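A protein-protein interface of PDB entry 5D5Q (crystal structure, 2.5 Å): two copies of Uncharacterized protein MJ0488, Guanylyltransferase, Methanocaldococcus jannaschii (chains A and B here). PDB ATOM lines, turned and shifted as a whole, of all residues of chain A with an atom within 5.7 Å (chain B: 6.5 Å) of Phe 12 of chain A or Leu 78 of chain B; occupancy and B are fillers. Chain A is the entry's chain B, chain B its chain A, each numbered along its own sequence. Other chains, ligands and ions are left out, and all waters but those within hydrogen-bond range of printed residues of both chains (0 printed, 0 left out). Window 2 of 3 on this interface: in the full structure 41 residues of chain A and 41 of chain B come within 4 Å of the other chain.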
ATOM      1  N   ILE A   7     -35.556 -10.860  35.526  1.00  0.00           N
ATOM      2  CA  ILE A   7     -35.611 -10.808  34.067  1.00  0.00           C
ATOM      3  C   ILE A   7     -34.637  -9.755  33.537  1.00  0.00           C
ATOM      4  O   ILE A   7     -33.857 -10.020  32.611  1.00  0.00           O
ATOM      5  CB  ILE A   7     -37.033 -10.519  33.548  1.00  0.00           C
ATOM      6  CG1 ILE A   7     -37.962 -11.695  33.849  1.00  0.00           C
ATOM      7  CG2 ILE A   7     -37.015 -10.363  32.054  1.00  0.00           C
ATOM      8  CD1 ILE A   7     -38.863 -11.496  35.032  1.00  0.00           C
ATOM      9  N   ILE A   8     -34.670  -8.571  34.141  1.00  0.00           N
ATOM     10  CA  ILE A   8     -33.762  -7.504  33.749  1.00  0.00           C
ATOM     11  C   ILE A   8     -32.311  -7.917  33.984  1.00  0.00           C
ATOM     12  O   ILE A   8     -31.444  -7.643  33.154  1.00  0.00           O
ATOM     13  CB  ILE A   8     -34.051  -6.197  34.522  1.00  0.00           C
ATOM     14  CG1 ILE A   8     -35.402  -5.616  34.105  1.00  0.00           C
ATOM     15  CG2 ILE A   8     -32.955  -5.172  34.282  1.00  0.00           C
ATOM     16  CD1 ILE A   8     -35.717  -4.291  34.758  1.00  0.00           C
ATOM     17  N   LYS A   9     -32.054  -8.603  35.094  1.00  0.00           N
ATOM     18  CA  LYS A   9     -30.709  -9.100  35.372  1.00  0.00           C
ATOM     19  C   LYS A   9     -30.222 -10.070  34.299  1.00  0.00           C
ATOM     20  O   LYS A   9     -29.084  -9.974  33.854  1.00  0.00           O
ATOM     21  CB  LYS A   9     -30.640  -9.763  36.749  1.00  0.00           C
ATOM     22  CG  LYS A   9     -29.219 -10.115  37.172  1.00  0.00           C
ATOM     23  CD  LYS A   9     -29.156 -10.659  38.591  1.00  0.00           C
ATOM     24  CE  LYS A   9     -30.276 -11.637  38.875  1.00  0.00           C
ATOM     25  NZ  LYS A   9     -30.293 -12.033  40.311  1.00  0.00           N
ATOM     26  N   LYS A  10     -31.076 -11.008  33.896  1.00  0.00           N
ATOM     27  CA  LYS A  10     -30.744 -11.930  32.811  1.00  0.00           C
ATOM     28  C   LYS A  10     -30.437 -11.179  31.520  1.00  0.00           C
ATOM     29  O   LYS A  10     -29.464 -11.494  30.831  1.00  0.00           O
ATOM     30  CB  LYS A  10     -31.868 -12.943  32.584  1.00  0.00           C
ATOM     31  CG  LYS A  10     -32.169 -13.813  33.795  1.00  0.00           C
ATOM     32  CD  LYS A  10     -33.074 -14.978  33.426  1.00  0.00           C
ATOM     33  CE  LYS A  10     -33.673 -15.634  34.661  1.00  0.00           C
ATOM     34  NZ  LYS A  10     -34.489 -14.684  35.466  1.00  0.00           N
ATOM     35  N   ALA A  11     -31.271 -10.195  31.192  1.00  0.00           N
ATOM     36  CA  ALA A  11     -31.047  -9.383  29.995  1.00  0.00           C
ATOM     37  C   ALA A  11     -29.669  -8.722  30.047  1.00  0.00           C
ATOM     38  O   ALA A  11     -28.905  -8.753  29.073  1.00  0.00           O
ATOM     39  CB  ALA A  11     -32.136  -8.336  29.851  1.00  0.00           C
ATOM     40  N   PHE A  12     -29.356  -8.141  31.202  1.00  0.00           N
ATOM     41  CA  PHE A  12     -28.080  -7.466  31.410  1.00  0.00           C
ATOM     42  C   PHE A  12     -26.919  -8.447  31.284  1.00  0.00           C
ATOM     43  O   PHE A  12     -25.870  -8.106  30.749  1.00  0.00           O
ATOM     44  CB  PHE A  12     -28.040  -6.787  32.784  1.00  0.00           C
ATOM     45  CG  PHE A  12     -28.830  -5.506  32.862  1.00  0.00           C
ATOM     46  CD1 PHE A  12     -29.617  -5.085  31.803  1.00  0.00           C
ATOM     47  CD2 PHE A  12     -28.772  -4.717  34.001  1.00  0.00           C
ATOM     48  CE1 PHE A  12     -30.335  -3.905  31.881  1.00  0.00           C
ATOM     49  CE2 PHE A  12     -29.488  -3.537  34.084  1.00  0.00           C
ATOM     50  CZ  PHE A  12     -30.270  -3.131  33.023  1.00  0.00           C
ATOM     51  N   ILE A  13     -27.112  -9.659  31.796  1.00  0.00           N
ATOM     52  CA  ILE A  13     -26.116 -10.721  31.686  1.00  0.00           C
ATOM     53  C   ILE A  13     -25.849 -11.074  30.225  1.00  0.00           C
ATOM     54  O   ILE A  13     -24.694 -11.212  29.815  1.00  0.00           O
ATOM     55  CB  ILE A  13     -26.556 -11.987  32.452  1.00  0.00           C
ATOM     56  CG1 ILE A  13     -26.483 -11.745  33.961  1.00  0.00           C
ATOM     57  CG2 ILE A  13     -25.683 -13.174  32.079  1.00  0.00           C
ATOM     58  CD1 ILE A  13     -27.025 -12.887  34.790  1.00  0.00           C
ATOM     59  N   GLU A  14     -26.918 -11.213  29.442  1.00  0.00           N
ATOM     60  CA  GLU A  14     -26.781 -11.467  28.011  1.00  0.00           C
ATOM     61  C   GLU A  14     -26.009 -10.339  27.339  1.00  0.00           C
ATOM     62  O   GLU A  14     -25.196 -10.577  26.445  1.00  0.00           O
ATOM     63  CB  GLU A  14     -28.144 -11.635  27.339  1.00  0.00           C
ATOM     64  CG  GLU A  14     -28.958 -12.812  27.843  1.00  0.00           C
ATOM     65  CD  GLU A  14     -30.213 -13.035  27.022  1.00  0.00           C
ATOM     66  OE1 GLU A  14     -30.768 -12.045  26.500  1.00  0.00           O
ATOM     67  OE2 GLU A  14     -30.642 -14.201  26.893  1.00  0.00           O
ATOM     68  N   SER A  15     -26.268  -9.110  27.772  1.00  0.00           N
ATOM     69  CA  SER A  15     -25.554  -7.965  27.217  1.00  0.00           C
ATOM     70  C   SER A  15     -24.066  -8.012  27.573  1.00  0.00           C
ATOM     71  O   SER A  15     -23.215  -7.709  26.738  1.00  0.00           O
ATOM     72  CB  SER A  15     -26.176  -6.658  27.707  1.00  0.00           C
ATOM     73  OG  SER A  15     -27.404  -6.400  27.048  1.00  0.00           O
ATOM     74  N   ILE A  16     -23.761  -8.390  28.812  1.00  0.00           N
ATOM     75  CA  ILE A  16     -22.379  -8.503  29.273  1.00  0.00           C
ATOM     76  C   ILE A  16     -21.621  -9.554  28.468  1.00  0.00           C
ATOM     77  O   ILE A  16     -20.492  -9.319  28.034  1.00  0.00           O
ATOM     78  CB  ILE A  16     -22.310  -8.855  30.772  1.00  0.00           C
ATOM     79  CG1 ILE A  16     -22.758  -7.660  31.612  1.00  0.00           C
ATOM     80  CG2 ILE A  16     -20.899  -9.262  31.169  1.00  0.00           C
ATOM     81  CD1 ILE A  16     -23.052  -8.005  33.048  1.00  0.00           C
ATOM     82  N   ASN A  17     -22.252 -10.704  28.254  1.00  0.00           N
ATOM     83  CA  ASN A  17     -21.617 -11.781  27.508  1.00  0.00           C
ATOM     84  C   ASN A  17     -21.751 -11.547  26.007  1.00  0.00           C
ATOM     85  O   ASN A  17     -21.334 -12.373  25.194  1.00  0.00           O
ATOM     86  CB  ASN A  17     -22.221 -13.132  27.895  1.00  0.00           C
ATOM     87  CG  ASN A  17     -22.040 -13.453  29.367  1.00  0.00           C
ATOM     88  OD1 ASN A  17     -23.007 -13.717  30.080  1.00  0.00           O
ATOM     89  ND2 ASN A  17     -20.794 -13.434  29.828  1.00  0.00           N
ATOM     90  N   ARG B  74     -22.491  -1.266  23.300  1.00  0.00           N
ATOM     91  CA  ARG B  74     -23.334  -2.186  24.046  1.00  0.00           C
ATOM     92  C   ARG B  74     -23.259  -1.653  25.469  1.00  0.00           C
ATOM     93  O   ARG B  74     -24.113  -1.949  26.299  1.00  0.00           O
ATOM     94  CB  ARG B  74     -22.897  -3.648  23.935  1.00  0.00           C
ATOM     95  CG  ARG B  74     -22.109  -4.202  25.097  1.00  0.00           C
ATOM     96  CD  ARG B  74     -21.643  -5.608  24.758  1.00  0.00           C
ATOM     97  NE  ARG B  74     -20.606  -6.091  25.663  1.00  0.00           N
ATOM     98  CZ  ARG B  74     -19.308  -5.889  25.485  1.00  0.00           C
ATOM     99  NH1 ARG B  74     -18.889  -5.202  24.433  1.00  0.00           N
ATOM    100  NH2 ARG B  74     -18.431  -6.371  26.357  1.00  0.00           N
ATOM    101  N   PHE B  75     -22.220  -0.852  25.727  1.00  0.00           N
ATOM    102  CA  PHE B  75     -22.002  -0.172  27.011  1.00  0.00           C
ATOM    103  C   PHE B  75     -23.126   0.792  27.402  1.00  0.00           C
ATOM    104  O   PHE B  75     -22.909   1.720  28.181  1.00  0.00           O
ATOM    105  CB  PHE B  75     -20.678   0.603  26.993  1.00  0.00           C
ATOM    106  CG  PHE B  75     -19.510  -0.144  27.584  1.00  0.00           C
ATOM    107  CD1 PHE B  75     -18.867  -1.160  26.894  1.00  0.00           C
ATOM    108  CD2 PHE B  75     -19.034   0.210  28.834  1.00  0.00           C
ATOM    109  CE1 PHE B  75     -17.788  -1.822  27.461  1.00  0.00           C
ATOM    110  CE2 PHE B  75     -17.955  -0.440  29.401  1.00  0.00           C
ATOM    111  CZ  PHE B  75     -17.333  -1.457  28.719  1.00  0.00           C
ATOM    112  N   ALA B  76     -24.313   0.589  26.843  1.00  0.00           N
ATOM    113  CA  ALA B  76     -25.452   1.450  27.119  1.00  0.00           C
ATOM    114  C   ALA B  76     -26.693   0.593  27.306  1.00  0.00           C
ATOM    115  O   ALA B  76     -27.741   1.078  27.731  1.00  0.00           O
ATOM    116  CB  ALA B  76     -25.652   2.449  25.994  1.00  0.00           C
ATOM    117  N   ASP B  77     -26.562  -0.689  26.982  1.00  0.00           N
ATOM    118  CA  ASP B  77     -27.678  -1.619  27.055  1.00  0.00           C
ATOM    119  C   ASP B  77     -27.977  -2.043  28.494  1.00  0.00           C
ATOM    120  O   ASP B  77     -28.894  -2.826  28.739  1.00  0.00           O
ATOM    121  CB  ASP B  77     -27.393  -2.850  26.190  1.00  0.00           C
ATOM    122  CG  ASP B  77     -27.203  -2.500  24.725  1.00  0.00           C
ATOM    123  OD1 ASP B  77     -27.718  -1.447  24.293  1.00  0.00           O
ATOM    124  OD2 ASP B  77     -26.536  -3.275  24.005  1.00  0.00           O
ATOM    125  N   LEU B  78     -27.195  -1.529  29.441  1.00  0.00           N
ATOM    126  CA  LEU B  78     -27.458  -1.768  30.859  1.00  0.00           C
ATOM    127  C   LEU B  78     -27.984  -0.520  31.563  1.00  0.00           C
ATOM    128  O   LEU B  78     -28.294  -0.557  32.754  1.00  0.00           O
ATOM    129  CB  LEU B  78     -26.191  -2.252  31.573  1.00  0.00           C
ATOM    130  CG  LEU B  78     -25.841  -3.742  31.570  1.00  0.00           C
ATOM    131  CD1 LEU B  78     -25.458  -4.212  30.178  1.00  0.00           C
ATOM    132  CD2 LEU B  78     -24.727  -4.035  32.564  1.00  0.00           C
ATOM    133  N   THR B  79     -28.094   0.582  30.826  1.00  0.00           N
ATOM    134  CA  THR B  79     -28.578   1.833  31.403  1.00  0.00           C
ATOM    135  C   THR B  79     -30.085   1.982  31.221  1.00  0.00           C
ATOM    136  O   THR B  79     -30.712   1.213  30.492  1.00  0.00           O
ATOM    137  CB  THR B  79     -27.860   3.055  30.793  1.00  0.00           C
ATOM    138  OG1 THR B  79     -28.268   3.231  29.431  1.00  0.00           O
ATOM    139  CG2 THR B  79     -26.351   2.868  30.850  1.00  0.00           C
ATOM    140  N   ARG B  80     -30.660   2.975  31.893  1.00  0.00           N
ATOM    141  CA  ARG B  80     -32.110   3.146  31.920  1.00  0.00           C
ATOM    142  C   ARG B  80     -32.701   3.519  30.561  1.00  0.00           C
ATOM    143  O   ARG B  80     -33.797   3.079  30.225  1.00  0.00           O
ATOM    144  CB  ARG B  80     -32.496   4.191  32.968  1.00  0.00           C
ATOM    145  CG  ARG B  80     -32.417   3.663  34.392  1.00  0.00           C
ATOM    146  CD  ARG B  80     -33.674   2.880  34.732  1.00  0.00           C
ATOM    147  NE  ARG B  80     -33.635   2.304  36.074  1.00  0.00           N
ATOM    148  CZ  ARG B  80     -34.158   2.878  37.151  1.00  0.00           C
ATOM    149  NH1 ARG B  80     -34.760   4.055  37.056  1.00  0.00           N
ATOM    150  NH2 ARG B  80     -34.077   2.273  38.328  1.00  0.00           N
ATOM    151  N   PRO B  82     -31.061   3.337  26.940  1.00  0.00           N
ATOM    152  CA  PRO B  82     -29.926   2.947  26.092  1.00  0.00           C
ATOM    153  C   PRO B  82     -29.673   3.832  24.866  1.00  0.00           C
ATOM    154  O   PRO B  82     -28.516   4.166  24.609  1.00  0.00           O
ATOM    155  CB  PRO B  82     -30.308   1.532  25.653  1.00  0.00           C
ATOM    156  CG  PRO B  82     -31.096   1.010  26.801  1.00  0.00           C
ATOM    157  CD  PRO B  82     -31.922   2.181  27.255  1.00  0.00           C
ATOM    158  N   ARG B 104     -32.656   0.660  22.509  1.00  0.00           N
ATOM    159  CA  ARG B 104     -33.842   0.351  23.292  1.00  0.00           C
ATOM    160  C   ARG B 104     -34.326   1.607  24.006  1.00  0.00           C
ATOM    161  O   ARG B 104     -33.521   2.422  24.457  1.00  0.00           O
ATOM    162  CB  ARG B 104     -33.560  -0.764  24.299  1.00  0.00           C
ATOM    163  CG  ARG B 104     -34.788  -1.209  25.075  1.00  0.00           C
ATOM    164  CD  ARG B 104     -34.494  -2.423  25.933  1.00  0.00           C
ATOM    165  NE  ARG B 104     -33.642  -2.096  27.070  1.00  0.00           N
ATOM    166  CZ  ARG B 104     -32.551  -2.775  27.404  1.00  0.00           C
ATOM    167  NH1 ARG B 104     -32.172  -3.822  26.685  1.00  0.00           N
ATOM    168  NH2 ARG B 104     -31.837  -2.407  28.459  1.00  0.00           N
ATOM    169  N   PRO B 108     -35.986  -3.525  29.327  1.00  0.00           N
ATOM    170  CA  PRO B 108     -36.129  -4.623  28.365  1.00  0.00           C
ATOM    171  C   PRO B 108     -37.591  -4.907  28.014  1.00  0.00           C
ATOM    172  O   PRO B 108     -38.401  -5.136  28.912  1.00  0.00           O
ATOM    173  CB  PRO B 108     -35.505  -5.807  29.103  1.00  0.00           C
ATOM    174  CG  PRO B 108     -34.462  -5.182  29.963  1.00  0.00           C
ATOM    175  CD  PRO B 108     -35.040  -3.863  30.407  1.00  0.00           C
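Among the printed residues, pairs that only touch across the chains: Ala 11 of chain A with Pro 108 of chain B (3.9 Å), Phe 12 of chain A with Asp 77 of chain B (3.6 Å), Phe 12 of chain A with Leu 78 of chain B (3.3 Å), Ser 15 of chain A with Asp 77 of chain B (3.7 Å), Ser 15 of chain A with Leu 78 of chain B (3.6 Å) and Ile 16 of chain A with Arg 74 of chain B (3.97 Å).
No position is printed for both chains.
O of Ser 15 of chain A is in hydrogen-bond range of NE of Arg 74 of chain B (3.3 Å).
The backbone carbonyl oxygen (O) of Asp 77 of chain B lies within hydrogen-bond range of the guanidinium group (NH2) of Arg 104 of chain B (3.0 Å).
The side-chain hydroxyl (OG) of Ser 15 of chain A sits at hydrogen-bond distance from the backbone carbonyl oxygen (O) of Ala 11 of chain A.
Printed residues of chain B that touch a printed residue of chain A: Arg 74, Asp 77, Leu 78 and Pro 108.
Of the 11 printed residues of chain A, 4 touch a printed residue of chain B.
Printed residues of chain A that touch a printed residue of chain B: Ala 11, Phe 12, Ser 15 and Ile 16.
Along chain A the printed residues that touch a printed residue of chain B span positions 11 to 16.
Of the printed residues of chain B, Ala 11 of chain A touches Pro 108 (3.9 Å).
Phe 12 of chain A touches two residues of chain B.
Of the printed residues of chain B, Ser 15 of chain A touches Arg 74 (3.3 Å), Asp 77 (3.7 Å) and Leu 78 (3.6 Å).
Asn 17 of chain A touches none of the printed residues of chain B.
Of the printed residues of chain A, Arg 74 of chain B touches Ser 15 and Ile 16.
Ala 76 of chain B touches none of the printed residues of chain A.
Printed residues of chain A within 4 Å of Asp 77 of chain B: Phe 12 and Ser 15.
Of the printed residues of chain A, Pro 108 of chain B touches Ala 11.
The nearest residue of chain B that does not touch Phe 12 of chain A is Arg 104 of chain B (4.03 Å).
The nearest printed residue of chain B that does not touch Ala 11 of chain A is Arg 104 of chain B (5.5 Å).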
